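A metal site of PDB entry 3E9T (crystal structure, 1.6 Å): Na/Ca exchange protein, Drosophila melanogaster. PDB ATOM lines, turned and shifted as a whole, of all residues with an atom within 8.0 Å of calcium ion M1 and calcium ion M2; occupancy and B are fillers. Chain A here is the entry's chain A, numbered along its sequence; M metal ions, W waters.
N of Glu 16 sits at hydrogen-bond distance from O of Leu 110 (2.8 Å). The side-chain carboxylate (OD2) of Asp 111 sits close to the backbone NH (N) of Glu 81 (3.4 Å). The side-chain amide nitrogen (ND2) of Asn 17 sits close to the side-chain carboxylate (OD2) of Asp 112 (3.2 Å).
Within 4 Å of calcium ion M1: Glu 16, Asp 76, Asp 77 and Asp 112.
Of the 17 residues printed, 5 come within 4 Å of calcium ion M2.
The side-chain carboxylate (OD1) of Asp 112 is bound to calcium ion M1, 2.2 Å away. OD2 of Asp 76 is bound to calcium ion M1 (2.3 Å). The side-chain carboxylate (OE2) of Glu 16 binds calcium ion M1, 2.4 Å away. Calcium ion M1 is bound by the backbone carbonyl oxygen (O) of Asp 77 (2.4 Å). Calcium ion M1 is bound by water W1 (2.7 Å).
Calcium ion M2 is bound by O of Val 79, OD2 of Asp 77, OE2 of Glu 16, OD1 of Asp 111, water W1 and OE1 of Glu 16. Slightly farther from calcium ion M2 lies OE1 of Glu 81 (3.0 Å).
Water W1 bridges the side-chain carboxylate of Asp 111 (3.2 Å) and the backbone carbonyl oxygen of Asp 78 (3.4 Å).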
ATOM      1  N   MET A  15     -10.297 -20.783 -15.652  1.00  0.00           N
ATOM      2  CA  MET A  15     -11.204 -19.738 -15.190  1.00  0.00           C
ATOM      3  C   MET A  15     -12.251 -19.470 -16.254  1.00  0.00           C
ATOM      4  O   MET A  15     -11.971 -19.567 -17.449  1.00  0.00           O
ATOM      5  CB  MET A  15     -10.436 -18.439 -14.874  1.00  0.00           C
ATOM      6  CG  MET A  15      -9.265 -18.662 -13.924  1.00  0.00           C
ATOM      7  SD  MET A  15      -9.778 -19.391 -12.346  1.00  0.00           S
ATOM      8  CE  MET A  15     -10.902 -18.179 -11.706  1.00  0.00           C
ATOM      9  N   GLU A  16     -13.450 -19.131 -15.805  1.00  0.00           N
ATOM     10  CA  GLU A  16     -14.580 -18.858 -16.691  1.00  0.00           C
ATOM     11  C   GLU A  16     -14.307 -17.783 -17.770  1.00  0.00           C
ATOM     12  O   GLU A  16     -14.915 -17.809 -18.843  1.00  0.00           O
ATOM     13  CB  GLU A  16     -15.784 -18.454 -15.854  1.00  0.00           C
ATOM     14  CG  GLU A  16     -17.024 -18.299 -16.684  1.00  0.00           C
ATOM     15  CD  GLU A  16     -18.183 -17.819 -15.880  1.00  0.00           C
ATOM     16  OE1 GLU A  16     -19.237 -18.484 -15.924  1.00  0.00           O
ATOM     17  OE2 GLU A  16     -18.045 -16.798 -15.172  1.00  0.00           O
ATOM     18  N   ASN A  17     -13.422 -16.852 -17.467  1.00  0.00           N
ATOM     19  CA  ASN A  17     -13.139 -15.717 -18.363  1.00  0.00           C
ATOM     20  C   ASN A  17     -11.849 -15.911 -19.149  1.00  0.00           C
ATOM     21  O   ASN A  17     -11.221 -14.941 -19.573  1.00  0.00           O
ATOM     22  CB  ASN A  17     -13.096 -14.402 -17.562  1.00  0.00           C
ATOM     23  CG  ASN A  17     -11.946 -14.355 -16.556  1.00  0.00           C
ATOM     24  OD1 ASN A  17     -11.458 -15.381 -16.075  1.00  0.00           O
ATOM     25  ND2 ASN A  17     -11.494 -13.143 -16.249  1.00  0.00           N
ATOM     26  N   CYS A  18     -11.444 -17.176 -19.338  1.00  0.00           N
ATOM     27  CA  CYS A  18     -10.176 -17.458 -19.997  1.00  0.00           C
ATOM     28  C   CYS A  18     -10.255 -17.274 -21.515  1.00  0.00           C
ATOM     29  O   CYS A  18      -9.227 -17.143 -22.163  1.00  0.00           O
ATOM     30  CB  CYS A  18      -9.682 -18.874 -19.682  1.00  0.00           C
ATOM     31  SG  CYS A  18     -10.653 -20.222 -20.434  1.00  0.00           S
ATOM     32  N   ASP A  51     -21.740 -23.042 -20.881  1.00  0.00           N
ATOM     33  CA  ASP A  51     -20.477 -22.954 -20.141  1.00  0.00           C
ATOM     34  C   ASP A  51     -19.240 -23.067 -21.027  1.00  0.00           C
ATOM     35  O   ASP A  51     -18.165 -22.550 -20.685  1.00  0.00           O
ATOM     36  CB  ASP A  51     -20.426 -24.046 -19.059  1.00  0.00           C
ATOM     37  CG  ASP A  51     -21.547 -23.922 -18.076  1.00  0.00           C
ATOM     38  OD1 ASP A  51     -22.411 -24.838 -17.977  1.00  0.00           O
ATOM     39  OD2 ASP A  51     -21.599 -22.865 -17.397  1.00  0.00           O
ATOM     40  N   ILE A  75     -17.337 -20.154 -22.201  1.00  0.00           N
ATOM     41  CA  ILE A  75     -18.327 -19.102 -22.255  1.00  0.00           C
ATOM     42  C   ILE A  75     -18.369 -18.394 -20.904  1.00  0.00           C
ATOM     43  O   ILE A  75     -18.596 -19.015 -19.866  1.00  0.00           O
ATOM     44  CB  ILE A  75     -19.734 -19.649 -22.650  1.00  0.00           C
ATOM     45  CG1 ILE A  75     -19.694 -20.291 -24.051  1.00  0.00           C
ATOM     46  CG2 ILE A  75     -20.792 -18.534 -22.598  1.00  0.00           C
ATOM     47  CD1 ILE A  75     -20.931 -21.026 -24.442  1.00  0.00           C
ATOM     48  N   ASP A  76     -18.141 -17.086 -20.949  1.00  0.00           N
ATOM     49  CA  ASP A  76     -18.146 -16.237 -19.757  1.00  0.00           C
ATOM     50  C   ASP A  76     -19.537 -15.636 -19.564  1.00  0.00           C
ATOM     51  O   ASP A  76     -20.224 -15.321 -20.535  1.00  0.00           O
ATOM     52  CB  ASP A  76     -17.111 -15.116 -19.929  1.00  0.00           C
ATOM     53  CG  ASP A  76     -16.746 -14.418 -18.611  1.00  0.00           C
ATOM     54  OD1 ASP A  76     -16.095 -13.358 -18.679  1.00  0.00           O
ATOM     55  OD2 ASP A  76     -17.099 -14.925 -17.517  1.00  0.00           O
ATOM     56  N   ASP A  77     -19.949 -15.503 -18.310  1.00  0.00           N
ATOM     57  CA  ASP A  77     -21.147 -14.728 -17.988  1.00  0.00           C
ATOM     58  C   ASP A  77     -20.920 -13.932 -16.705  1.00  0.00           C
ATOM     59  O   ASP A  77     -19.818 -13.943 -16.140  1.00  0.00           O
ATOM     60  CB  ASP A  77     -22.383 -15.617 -17.901  1.00  0.00           C
ATOM     61  CG  ASP A  77     -22.248 -16.729 -16.875  1.00  0.00           C
ATOM     62  OD1 ASP A  77     -22.688 -17.845 -17.177  1.00  0.00           O
ATOM     63  OD2 ASP A  77     -21.703 -16.489 -15.769  1.00  0.00           O
ATOM     64  N   ASP A  78     -21.965 -13.234 -16.242  1.00  0.00           N
ATOM     65  CA  ASP A  78     -21.887 -12.496 -14.990  1.00  0.00           C
ATOM     66  C   ASP A  78     -22.418 -13.267 -13.780  1.00  0.00           C
ATOM     67  O   ASP A  78     -22.162 -12.890 -12.641  1.00  0.00           O
ATOM     68  CB  ASP A  78     -22.578 -11.139 -15.115  1.00  0.00           C
ATOM     69  CG  ASP A  78     -21.615 -10.016 -15.429  1.00  0.00           C
ATOM     70  OD1 ASP A  78     -20.608 -10.278 -16.129  1.00  0.00           O
ATOM     71  OD2 ASP A  78     -21.862  -8.861 -14.993  1.00  0.00           O
ATOM     72  N   VAL A  79     -23.160 -14.345 -14.045  1.00  0.00           N
ATOM     73  CA  VAL A  79     -23.810 -15.101 -12.965  1.00  0.00           C
ATOM     74  C   VAL A  79     -22.804 -15.940 -12.169  1.00  0.00           C
ATOM     75  O   VAL A  79     -21.924 -16.571 -12.735  1.00  0.00           O
ATOM     76  CB  VAL A  79     -24.942 -15.993 -13.515  1.00  0.00           C
ATOM     77  CG1 VAL A  79     -25.717 -16.662 -12.368  1.00  0.00           C
ATOM     78  CG2 VAL A  79     -25.896 -15.175 -14.390  1.00  0.00           C
ATOM     79  N   PHE A  80     -22.960 -15.907 -10.841  1.00  0.00           N
ATOM     80  CA  PHE A  80     -22.185 -16.732  -9.926  1.00  0.00           C
ATOM     81  C   PHE A  80     -22.497 -18.210 -10.120  1.00  0.00           C
ATOM     82  O   PHE A  80     -23.661 -18.598 -10.217  1.00  0.00           O
ATOM     83  CB  PHE A  80     -22.510 -16.284  -8.486  1.00  0.00           C
ATOM     84  CG  PHE A  80     -21.913 -17.164  -7.409  1.00  0.00           C
ATOM     85  CD1 PHE A  80     -22.736 -17.994  -6.645  1.00  0.00           C
ATOM     86  CD2 PHE A  80     -20.544 -17.142  -7.147  1.00  0.00           C
ATOM     87  CE1 PHE A  80     -22.212 -18.800  -5.631  1.00  0.00           C
ATOM     88  CE2 PHE A  80     -20.001 -17.951  -6.144  1.00  0.00           C
ATOM     89  CZ  PHE A  80     -20.834 -18.777  -5.379  1.00  0.00           C
ATOM     90  N   GLU A  81     -21.460 -19.027 -10.244  1.00  0.00           N
ATOM     91  CA  GLU A  81     -21.649 -20.470 -10.354  1.00  0.00           C
ATOM     92  C   GLU A  81     -20.627 -21.179  -9.498  1.00  0.00           C
ATOM     93  O   GLU A  81     -19.516 -20.686  -9.301  1.00  0.00           O
ATOM     94  CB  GLU A  81     -21.495 -20.952 -11.806  1.00  0.00           C
ATOM     95  CG  GLU A  81     -22.604 -20.488 -12.737  1.00  0.00           C
ATOM     96  CD  GLU A  81     -22.120 -20.405 -14.173  1.00  0.00           C
ATOM     97  OE1 GLU A  81     -21.810 -19.275 -14.621  1.00  0.00           O
ATOM     98  OE2 GLU A  81     -22.033 -21.454 -14.847  1.00  0.00           O
ATOM     99  N   GLU A  82     -21.014 -22.329  -8.987  1.00  0.00           N
ATOM    100  CA  GLU A  82     -20.080 -23.200  -8.304  1.00  0.00           C
ATOM    101  C   GLU A  82     -19.131 -23.821  -9.333  1.00  0.00           C
ATOM    102  O   GLU A  82     -19.370 -23.704 -10.532  1.00  0.00           O
ATOM    103  CB  GLU A  82     -20.859 -24.275  -7.532  1.00  0.00           C
ATOM    104  CG  GLU A  82     -21.834 -23.630  -6.539  1.00  0.00           C
ATOM    105  CD  GLU A  82     -22.723 -24.620  -5.796  1.00  0.00           C
ATOM    106  OE1 GLU A  82     -22.624 -25.842  -6.042  1.00  0.00           O
ATOM    107  OE2 GLU A  82     -23.541 -24.167  -4.951  1.00  0.00           O
ATOM    108  N   ILE A 109     -14.228 -25.806 -14.648  1.00  0.00           N
ATOM    109  CA  ILE A 109     -14.332 -24.364 -14.813  1.00  0.00           C
ATOM    110  C   ILE A 109     -14.555 -23.694 -13.455  1.00  0.00           C
ATOM    111  O   ILE A 109     -15.495 -24.048 -12.724  1.00  0.00           O
ATOM    112  CB  ILE A 109     -15.507 -23.968 -15.740  1.00  0.00           C
ATOM    113  CG1 ILE A 109     -15.385 -24.657 -17.101  1.00  0.00           C
ATOM    114  CG2 ILE A 109     -15.581 -22.439 -15.892  1.00  0.00           C
ATOM    115  CD1 ILE A 109     -16.692 -24.576 -17.940  1.00  0.00           C
ATOM    116  N   LEU A 110     -13.684 -22.749 -13.115  1.00  0.00           N
ATOM    117  CA  LEU A 110     -13.881 -21.940 -11.906  1.00  0.00           C
ATOM    118  C   LEU A 110     -14.507 -20.597 -12.257  1.00  0.00           C
ATOM    119  O   LEU A 110     -14.042 -19.922 -13.164  1.00  0.00           O
ATOM    120  CB  LEU A 110     -12.551 -21.714 -11.176  1.00  0.00           C
ATOM    121  CG  LEU A 110     -11.656 -22.947 -11.003  1.00  0.00           C
ATOM    122  CD1 LEU A 110     -10.370 -22.561 -10.323  1.00  0.00           C
ATOM    123  CD2 LEU A 110     -12.352 -24.062 -10.210  1.00  0.00           C
ATOM    124  N   ASP A 111     -15.549 -20.225 -11.519  1.00  0.00           N
ATOM    125  CA  ASP A 111     -16.216 -18.937 -11.721  1.00  0.00           C
ATOM    126  C   ASP A 111     -15.315 -17.765 -11.295  1.00  0.00           C
ATOM    127  O   ASP A 111     -14.468 -17.905 -10.398  1.00  0.00           O
ATOM    128  CB  ASP A 111     -17.511 -18.919 -10.916  1.00  0.00           C
ATOM    129  CG  ASP A 111     -18.607 -18.091 -11.572  1.00  0.00           C
ATOM    130  OD1 ASP A 111     -19.191 -18.561 -12.573  1.00  0.00           O
ATOM    131  OD2 ASP A 111     -18.883 -16.971 -11.076  1.00  0.00           O
ATOM    132  N   ASP A 112     -15.481 -16.625 -11.961  1.00  0.00           N
ATOM    133  CA  ASP A 112     -14.777 -15.397 -11.611  1.00  0.00           C
ATOM    134  C   ASP A 112     -15.819 -14.318 -11.283  1.00  0.00           C
ATOM    135  O   ASP A 112     -15.744 -13.674 -10.248  1.00  0.00           O
ATOM    136  CB  ASP A 112     -13.902 -14.929 -12.773  1.00  0.00           C
ATOM    137  CG  ASP A 112     -14.713 -14.499 -13.977  1.00  0.00           C
ATOM    138  OD1 ASP A 112     -15.788 -15.093 -14.241  1.00  0.00           O
ATOM    139  OD2 ASP A 112     -14.290 -13.553 -14.668  1.00  0.00           O
HETATM  140 CA    CA M   1     -17.621 -14.457 -15.312  1.00  0.00          CA
HETATM  141 CA    CA M   2     -20.167 -16.850 -14.026  1.00  0.00          CA
HETATM  142  O   HOH W   1     -19.320 -14.686 -13.245  1.00  0.00           O
